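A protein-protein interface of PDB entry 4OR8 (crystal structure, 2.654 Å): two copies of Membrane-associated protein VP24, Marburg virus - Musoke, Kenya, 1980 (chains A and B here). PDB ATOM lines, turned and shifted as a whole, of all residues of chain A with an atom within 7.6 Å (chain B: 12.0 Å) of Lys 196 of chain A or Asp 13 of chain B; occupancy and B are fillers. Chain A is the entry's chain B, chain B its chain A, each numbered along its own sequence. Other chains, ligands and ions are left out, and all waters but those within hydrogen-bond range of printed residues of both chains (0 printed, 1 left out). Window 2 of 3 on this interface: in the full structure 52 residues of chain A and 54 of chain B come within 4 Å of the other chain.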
ATOM      1  N   LYS A 117      -7.610  19.268  25.082  1.00  0.00           N
ATOM      2  CA  LYS A 117      -8.043  18.393  23.996  1.00  0.00           C
ATOM      3  C   LYS A 117      -9.476  18.693  23.568  1.00  0.00           C
ATOM      4  O   LYS A 117     -10.044  17.950  22.774  1.00  0.00           O
ATOM      5  CB  LYS A 117      -7.892  16.908  24.357  1.00  0.00           C
ATOM      6  CG  LYS A 117      -6.463  16.480  24.677  1.00  0.00           C
ATOM      7  CD  LYS A 117      -5.508  16.750  23.519  1.00  0.00           C
ATOM      8  CE  LYS A 117      -5.839  15.876  22.316  1.00  0.00           C
ATOM      9  NZ  LYS A 117      -4.945  16.159  21.158  1.00  0.00           N
ATOM     10  N   LEU A 141      -1.366  15.338  31.754  1.00  0.00           N
ATOM     11  CA  LEU A 141      -2.113  14.155  32.168  1.00  0.00           C
ATOM     12  C   LEU A 141      -1.232  13.057  32.756  1.00  0.00           C
ATOM     13  O   LEU A 141      -1.631  12.374  33.698  1.00  0.00           O
ATOM     14  CB  LEU A 141      -2.920  13.591  30.994  1.00  0.00           C
ATOM     15  CG  LEU A 141      -4.092  14.431  30.485  1.00  0.00           C
ATOM     16  CD1 LEU A 141      -4.661  13.837  29.211  1.00  0.00           C
ATOM     17  CD2 LEU A 141      -5.167  14.536  31.548  1.00  0.00           C
ATOM     18  N   GLU A 194     -17.226  12.425  30.292  1.00  0.00           N
ATOM     19  CA  GLU A 194     -16.271  11.330  30.168  1.00  0.00           C
ATOM     20  C   GLU A 194     -15.419  11.492  28.925  1.00  0.00           C
ATOM     21  O   GLU A 194     -15.862  12.046  27.924  1.00  0.00           O
ATOM     22  CB  GLU A 194     -16.989   9.986  30.128  1.00  0.00           C
ATOM     23  CG  GLU A 194     -17.945   9.769  31.279  1.00  0.00           C
ATOM     24  CD  GLU A 194     -18.469   8.354  31.330  1.00  0.00           C
ATOM     25  OE1 GLU A 194     -17.934   7.499  30.593  1.00  0.00           O
ATOM     26  OE2 GLU A 194     -19.415   8.099  32.106  1.00  0.00           O
ATOM     27  N   ILE A 195     -14.191  10.997  28.996  1.00  0.00           N
ATOM     28  CA  ILE A 195     -13.273  11.071  27.873  1.00  0.00           C
ATOM     29  C   ILE A 195     -12.189  10.005  28.018  1.00  0.00           C
ATOM     30  O   ILE A 195     -11.852   9.601  29.131  1.00  0.00           O
ATOM     31  CB  ILE A 195     -12.643  12.483  27.771  1.00  0.00           C
ATOM     32  CG1 ILE A 195     -11.906  12.662  26.443  1.00  0.00           C
ATOM     33  CG2 ILE A 195     -11.723  12.753  28.950  1.00  0.00           C
ATOM     34  CD1 ILE A 195     -11.428  14.070  26.202  1.00  0.00           C
ATOM     35  N   LYS A 196     -11.678   9.521  26.890  1.00  0.00           N
ATOM     36  CA  LYS A 196     -10.495   8.668  26.889  1.00  0.00           C
ATOM     37  C   LYS A 196      -9.330   9.449  26.298  1.00  0.00           C
ATOM     38  O   LYS A 196      -9.465  10.062  25.243  1.00  0.00           O
ATOM     39  CB  LYS A 196     -10.724   7.392  26.078  1.00  0.00           C
ATOM     40  CG  LYS A 196     -11.486   6.298  26.802  1.00  0.00           C
ATOM     41  CD  LYS A 196     -12.985   6.539  26.765  1.00  0.00           C
ATOM     42  CE  LYS A 196     -13.751   5.320  27.251  1.00  0.00           C
ATOM     43  NZ  LYS A 196     -15.221   5.549  27.235  1.00  0.00           N
ATOM     44  N   LEU A 197      -8.194   9.435  26.984  1.00  0.00           N
ATOM     45  CA  LEU A 197      -7.012  10.149  26.520  1.00  0.00           C
ATOM     46  C   LEU A 197      -5.744   9.388  26.886  1.00  0.00           C
ATOM     47  O   LEU A 197      -5.504   9.092  28.058  1.00  0.00           O
ATOM     48  CB  LEU A 197      -6.966  11.564  27.108  1.00  0.00           C
ATOM     49  CG  LEU A 197      -7.958  12.602  26.570  1.00  0.00           C
ATOM     50  CD1 LEU A 197      -7.848  13.917  27.334  1.00  0.00           C
ATOM     51  CD2 LEU A 197      -7.746  12.830  25.080  1.00  0.00           C
ATOM     52  N   THR A 198      -4.945   9.072  25.869  1.00  0.00           N
ATOM     53  CA  THR A 198      -3.670   8.367  26.033  1.00  0.00           C
ATOM     54  C   THR A 198      -3.749   7.114  26.908  1.00  0.00           C
ATOM     55  O   THR A 198      -2.872   6.870  27.735  1.00  0.00           O
ATOM     56  CB  THR A 198      -2.563   9.297  26.570  1.00  0.00           C
ATOM     57  OG1 THR A 198      -2.866   9.683  27.916  1.00  0.00           O
ATOM     58  CG2 THR A 198      -2.442  10.538  25.700  1.00  0.00           C
ATOM     59  N   GLY A 199      -4.803   6.328  26.722  1.00  0.00           N
ATOM     60  CA  GLY A 199      -4.929   5.051  27.399  1.00  0.00           C
ATOM     61  C   GLY A 199      -5.386   5.126  28.846  1.00  0.00           C
ATOM     62  O   GLY A 199      -5.007   4.285  29.663  1.00  0.00           O
ATOM     63  N   GLN A 200      -6.198   6.127  29.171  1.00  0.00           N
ATOM     64  CA  GLN A 200      -6.787   6.204  30.504  1.00  0.00           C
ATOM     65  C   GLN A 200      -8.124   6.940  30.536  1.00  0.00           C
ATOM     66  O   GLN A 200      -8.224   8.099  30.125  1.00  0.00           O
ATOM     67  CB  GLN A 200      -5.800   6.795  31.519  1.00  0.00           C
ATOM     68  CG  GLN A 200      -5.200   8.139  31.151  1.00  0.00           C
ATOM     69  CD  GLN A 200      -4.100   8.545  32.115  1.00  0.00           C
ATOM     70  OE1 GLN A 200      -3.096   7.847  32.255  1.00  0.00           O
ATOM     71  NE2 GLN A 200      -4.293   9.665  32.800  1.00  0.00           N
ATOM     72  N   GLN A 201      -9.148   6.250  31.030  1.00  0.00           N
ATOM     73  CA  GLN A 201     -10.496   6.797  31.077  1.00  0.00           C
ATOM     74  C   GLN A 201     -10.625   7.875  32.147  1.00  0.00           C
ATOM     75  O   GLN A 201     -10.420   7.615  33.330  1.00  0.00           O
ATOM     76  CB  GLN A 201     -11.512   5.687  31.339  1.00  0.00           C
ATOM     77  CG  GLN A 201     -12.941   6.088  31.024  1.00  0.00           C
ATOM     78  CD  GLN A 201     -13.954   5.070  31.506  1.00  0.00           C
ATOM     79  OE1 GLN A 201     -13.852   4.553  32.621  1.00  0.00           O
ATOM     80  NE2 GLN A 201     -14.941   4.776  30.668  1.00  0.00           N
ATOM     81  N   ILE A 202     -10.974   9.085  31.726  1.00  0.00           N
ATOM     82  CA  ILE A 202     -11.118  10.203  32.651  1.00  0.00           C
ATOM     83  C   ILE A 202     -12.576  10.637  32.767  1.00  0.00           C
ATOM     84  O   ILE A 202     -13.252  10.841  31.761  1.00  0.00           O
ATOM     85  CB  ILE A 202     -10.261  11.401  32.208  1.00  0.00           C
ATOM     86  CG1 ILE A 202      -8.800  10.975  32.052  1.00  0.00           C
ATOM     87  CG2 ILE A 202     -10.386  12.548  33.199  1.00  0.00           C
ATOM     88  CD1 ILE A 202      -7.891  12.084  31.575  1.00  0.00           C
ATOM     89  N   ILE A 203     -13.055  10.771  34.002  1.00  0.00           N
ATOM     90  CA  ILE A 203     -14.433  11.177  34.256  1.00  0.00           C
ATOM     91  C   ILE A 203     -14.526  12.349  35.230  1.00  0.00           C
ATOM     92  O   ILE A 203     -14.052  12.269  36.363  1.00  0.00           O
ATOM     93  CB  ILE A 203     -15.273  10.008  34.800  1.00  0.00           C
ATOM     94  CG1 ILE A 203     -15.481   8.953  33.712  1.00  0.00           C
ATOM     95  CG2 ILE A 203     -16.615  10.509  35.301  1.00  0.00           C
ATOM     96  CD1 ILE A 203     -14.845   7.616  34.012  1.00  0.00           C
ATOM     97  N   ARG A 216      -9.247   6.373  35.545  1.00  0.00           N
ATOM     98  CA  ARG A 216      -9.010   4.933  35.546  1.00  0.00           C
ATOM     99  C   ARG A 216      -7.923   4.596  34.536  1.00  0.00           C
ATOM    100  O   ARG A 216      -8.129   4.698  33.328  1.00  0.00           O
ATOM    101  CB  ARG A 216     -10.294   4.170  35.225  1.00  0.00           C
ATOM    102  CG  ARG A 216     -11.429   4.431  36.205  1.00  0.00           C
ATOM    103  CD  ARG A 216     -12.709   3.749  35.756  1.00  0.00           C
ATOM    104  NE  ARG A 216     -13.817   3.985  36.677  1.00  0.00           N
ATOM    105  CZ  ARG A 216     -15.043   3.499  36.508  1.00  0.00           C
ATOM    106  NH1 ARG A 216     -15.323   2.747  35.451  1.00  0.00           N
ATOM    107  NH2 ARG A 216     -15.991   3.765  37.396  1.00  0.00           N
ATOM    108  N   ASP B  12      -5.094   6.642  19.958  1.00  0.00           N
ATOM    109  CA  ASP B  12      -6.156   5.697  20.281  1.00  0.00           C
ATOM    110  C   ASP B  12      -6.959   6.181  21.483  1.00  0.00           C
ATOM    111  O   ASP B  12      -6.643   5.845  22.625  1.00  0.00           O
ATOM    112  CB  ASP B  12      -5.572   4.319  20.549  1.00  0.00           C
ATOM    113  N   ASP B  13      -8.002   6.964  21.220  1.00  0.00           N
ATOM    114  CA  ASP B  13      -8.765   7.600  22.289  1.00  0.00           C
ATOM    115  C   ASP B  13     -10.145   8.071  21.822  1.00  0.00           C
ATOM    116  O   ASP B  13     -10.358   8.317  20.636  1.00  0.00           O
ATOM    117  CB  ASP B  13      -7.975   8.767  22.860  1.00  0.00           C
ATOM    118  N   LYS B  14     -11.074   8.202  22.766  1.00  0.00           N
ATOM    119  CA  LYS B  14     -12.435   8.638  22.461  1.00  0.00           C
ATOM    120  C   LYS B  14     -12.572  10.161  22.517  1.00  0.00           C
ATOM    121  O   LYS B  14     -11.576  10.884  22.492  1.00  0.00           O
ATOM    122  CB  LYS B  14     -13.428   7.979  23.411  1.00  0.00           C
ATOM    123  N   MET B  15     -13.811  10.641  22.591  1.00  0.00           N
ATOM    124  CA  MET B  15     -14.081  12.073  22.660  1.00  0.00           C
ATOM    125  C   MET B  15     -14.924  12.411  23.886  1.00  0.00           C
ATOM    126  O   MET B  15     -15.515  11.523  24.500  1.00  0.00           O
ATOM    127  CB  MET B  15     -14.794  12.549  21.390  1.00  0.00           C
ATOM    128  CG  MET B  15     -16.253  12.116  21.288  1.00  0.00           C
ATOM    129  SD  MET B  15     -17.050  12.638  19.752  1.00  0.00           S
ATOM    130  CE  MET B  15     -16.685  14.393  19.751  1.00  0.00           C
ATOM    131  N   ALA B  16     -14.982  13.693  24.236  1.00  0.00           N
ATOM    132  CA  ALA B  16     -15.750  14.135  25.397  1.00  0.00           C
ATOM    133  C   ALA B  16     -17.256  13.967  25.188  1.00  0.00           C
ATOM    134  O   ALA B  16     -17.796  14.334  24.144  1.00  0.00           O
ATOM    135  CB  ALA B  16     -15.415  15.578  25.746  1.00  0.00           C
ATOM    136  N   GLU B  17     -17.925  13.411  26.192  1.00  0.00           N
ATOM    137  CA  GLU B  17     -19.352  13.136  26.108  1.00  0.00           C
ATOM    138  C   GLU B  17     -20.050  13.391  27.441  1.00  0.00           C
ATOM    139  O   GLU B  17     -19.543  13.022  28.502  1.00  0.00           O
ATOM    140  CB  GLU B  17     -19.585  11.689  25.662  1.00  0.00           C
ATOM    141  CG  GLU B  17     -18.836  10.658  26.498  1.00  0.00           C
ATOM    142  CD  GLU B  17     -19.049   9.235  26.013  1.00  0.00           C
ATOM    143  OE1 GLU B  17     -19.610   9.056  24.910  1.00  0.00           O
ATOM    144  OE2 GLU B  17     -18.658   8.294  26.737  1.00  0.00           O
ATOM    145  N   LEU B  18     -21.213  14.029  27.384  1.00  0.00           N
ATOM    146  CA  LEU B  18     -22.008  14.253  28.581  1.00  0.00           C
ATOM    147  C   LEU B  18     -22.604  12.934  29.054  1.00  0.00           C
ATOM    148  O   LEU B  18     -23.103  12.140  28.256  1.00  0.00           O
ATOM    149  CB  LEU B  18     -23.108  15.279  28.318  1.00  0.00           C
ATOM    150  CG  LEU B  18     -22.624  16.677  27.939  1.00  0.00           C
ATOM    151  CD1 LEU B  18     -23.809  17.589  27.684  1.00  0.00           C
ATOM    152  CD2 LEU B  18     -21.735  17.242  29.027  1.00  0.00           C
ATOM    153  N   SER B  19     -22.548  12.703  30.360  1.00  0.00           N
ATOM    154  CA  SER B  19     -22.896  11.405  30.918  1.00  0.00           C
ATOM    155  C   SER B  19     -23.763  11.519  32.164  1.00  0.00           C
ATOM    156  O   SER B  19     -23.495  12.328  33.054  1.00  0.00           O
ATOM    157  CB  SER B  19     -21.622  10.624  31.241  1.00  0.00           C
ATOM    158  OG  SER B  19     -21.874   9.615  32.200  1.00  0.00           O
ATOM    159  N   THR B  20     -24.803  10.697  32.221  1.00  0.00           N
ATOM    160  CA  THR B  20     -25.674  10.646  33.386  1.00  0.00           C
ATOM    161  C   THR B  20     -25.343   9.417  34.215  1.00  0.00           C
ATOM    162  O   THR B  20     -26.204   8.861  34.892  1.00  0.00           O
ATOM    163  CB  THR B  20     -27.160  10.608  32.978  1.00  0.00           C
ATOM    164  OG1 THR B  20     -27.364   9.569  32.010  1.00  0.00           O
ATOM    165  CG2 THR B  20     -27.578  11.939  32.373  1.00  0.00           C
ATOM    166  N   ARG B  21     -24.082   9.004  34.159  1.00  0.00           N
ATOM    167  CA  ARG B  21     -23.648   7.767  34.801  1.00  0.00           C
ATOM    168  C   ARG B  21     -23.873   7.762  36.309  1.00  0.00           C
ATOM    169  O   ARG B  21     -24.120   6.711  36.903  1.00  0.00           O
ATOM    170  CB  ARG B  21     -22.177   7.492  34.501  1.00  0.00           C
ATOM    171  CG  ARG B  21     -21.743   6.095  34.885  1.00  0.00           C
ATOM    172  CD  ARG B  21     -20.302   5.842  34.510  1.00  0.00           C
ATOM    173  NE  ARG B  21     -19.396   6.722  35.236  1.00  0.00           N
ATOM    174  CZ  ARG B  21     -18.108   6.458  35.428  1.00  0.00           C
ATOM    175  NH1 ARG B  21     -17.585   5.334  34.953  1.00  0.00           N
ATOM    176  NH2 ARG B  21     -17.347   7.311  36.102  1.00  0.00           N
ATOM    177  N   TYR B  22     -23.785   8.934  36.925  1.00  0.00           N
ATOM    178  CA  TYR B  22     -23.967   9.043  38.364  1.00  0.00           C
ATOM    179  C   TYR B  22     -25.311   9.657  38.717  1.00  0.00           C
ATOM    180  O   TYR B  22     -25.383  10.618  39.481  1.00  0.00           O
ATOM    181  CB  TYR B  22     -22.840   9.860  38.990  1.00  0.00           C
ATOM    182  CG  TYR B  22     -21.478   9.213  38.890  1.00  0.00           C
ATOM    183  CD1 TYR B  22     -21.176   8.070  39.616  1.00  0.00           C
ATOM    184  CD2 TYR B  22     -20.491   9.757  38.082  1.00  0.00           C
ATOM    185  CE1 TYR B  22     -19.927   7.479  39.531  1.00  0.00           C
ATOM    186  CE2 TYR B  22     -19.242   9.178  37.994  1.00  0.00           C
ATOM    187  CZ  TYR B  22     -18.965   8.041  38.720  1.00  0.00           C
ATOM    188  OH  TYR B  22     -17.718   7.469  38.628  1.00  0.00           O
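Among the printed residues, pairs that only touch across the chains: Glu 194 of chain A with Ala 16 of chain B (3.3 Å), Ile 195 of chain A with Met 15 of chain B (3.96 Å), Ile 195 of chain A with Ala 16 of chain B (3.9 Å), Lys 196 of chain A with Asp 13 of chain B (3.1 Å), Ile 203 of chain A with Arg 21 of chain B (3.3 Å) and Ile 203 of chain A with Tyr 22 of chain B (3.99 Å).
No position is printed for both chains.
Lys 117 of chain A touches none of the printed residues of chain B.
Of chain B, only Met 15 (3.96 Å) and Ala 16 (3.9 Å) come within 4 Å of Ile 195 of chain A.
Lys 196 of chain A touches just these residues of chain B: Asp 13 and Lys 14.
No residue of chain B comes within 4 Å of Thr 198 of chain A.
No residue of chain B comes within 4 Å of Gln 201 of chain A.
No residue of chain B comes within 4 Å of Ile 202 of chain A.
Of the printed residues of chain B, Arg 216 of chain A touches Arg 21 (3.3 Å).
Asp 12 of chain B touches none of the printed residues of chain A.
Of chain A, only Lys 196 comes within 4 Å of Asp 13 of chain B.
Printed residues of chain A within 4 Å of Met 15 of chain B: Glu 194 and Ile 195.
Of the printed residues of chain A, Glu 17 of chain B touches Glu 194 (3.0 Å).
Printed residues of chain A within 4 Å of Ser 19 of chain B: Glu 194.
Of the printed residues of chain A, Arg 21 of chain B touches Glu 194, Ile 203 and Arg 216.
The nearest residue of chain B that does not touch Lys 196 of chain A is Glu 17 of chain B (4.4 Å).
The nearest printed residue of chain A that does not touch Ser 19 of chain B is Ile 203 of chain A (6.2 Å).
Hydrophobic or aromatic side chains of chain B that line the printed part of chain A: Tyr 22.
Of the 13 printed residues of chain A, 5 touch a printed residue of chain B.
Among the printed residues, 12 pairs touch across the chains.
Among the printed residues, Asp or Glu carboxylates within 4 Å of a Lys or Arg side-chain nitrogen of the other chain: Glu 194 of chain A with Arg 21 of chain B (3.4 Å).
The backbone NH (N) of Lys 14 of chain B sits close to the backbone carbonyl oxygen (O) of Lys 196 of chain A (3.5 Å).
The backbone carbonyl oxygen (O) of Glu 17 of chain B sits at hydrogen-bond distance from the backbone NH (N) of Glu 194 of chain A (3.0 Å).
OG of Ser 19 of chain B lies within hydrogen-bond range of OE2 of Glu 194 of chain A.
NE of Arg 21 of chain B lies within salt-bridge range of OE2 of Glu 194 of chain A (3.4 Å).
O of Glu 194 of chain A lies close to O of Met 15 of chain B, at 3.5 Å.
The guanidinium group (NH1) of Arg 21 of chain B sits close to the guanidinium group (NH2) of Arg 216 of chain A, at 3.3 Å.
N of Arg 21 of chain B is in hydrogen-bond range of OG of Ser 19 of chain B (3.0 Å).
The guanidinium group (NH2) of Arg 21 of chain B is in hydrogen-bond range of the side-chain hydroxyl (OH) of Tyr 22 of chain B, 2.6 Å away.
The backbone carbonyl oxygen (O) of Ile 195 of chain A lies within hydrogen-bond range of the backbone NH (N) of Ile 202 of chain A (2.8 Å).
The backbone NH (N) of Arg 216 of chain A lies within hydrogen-bond range of the backbone carbonyl oxygen (O) of Gln 201 of chain A (2.8 Å).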
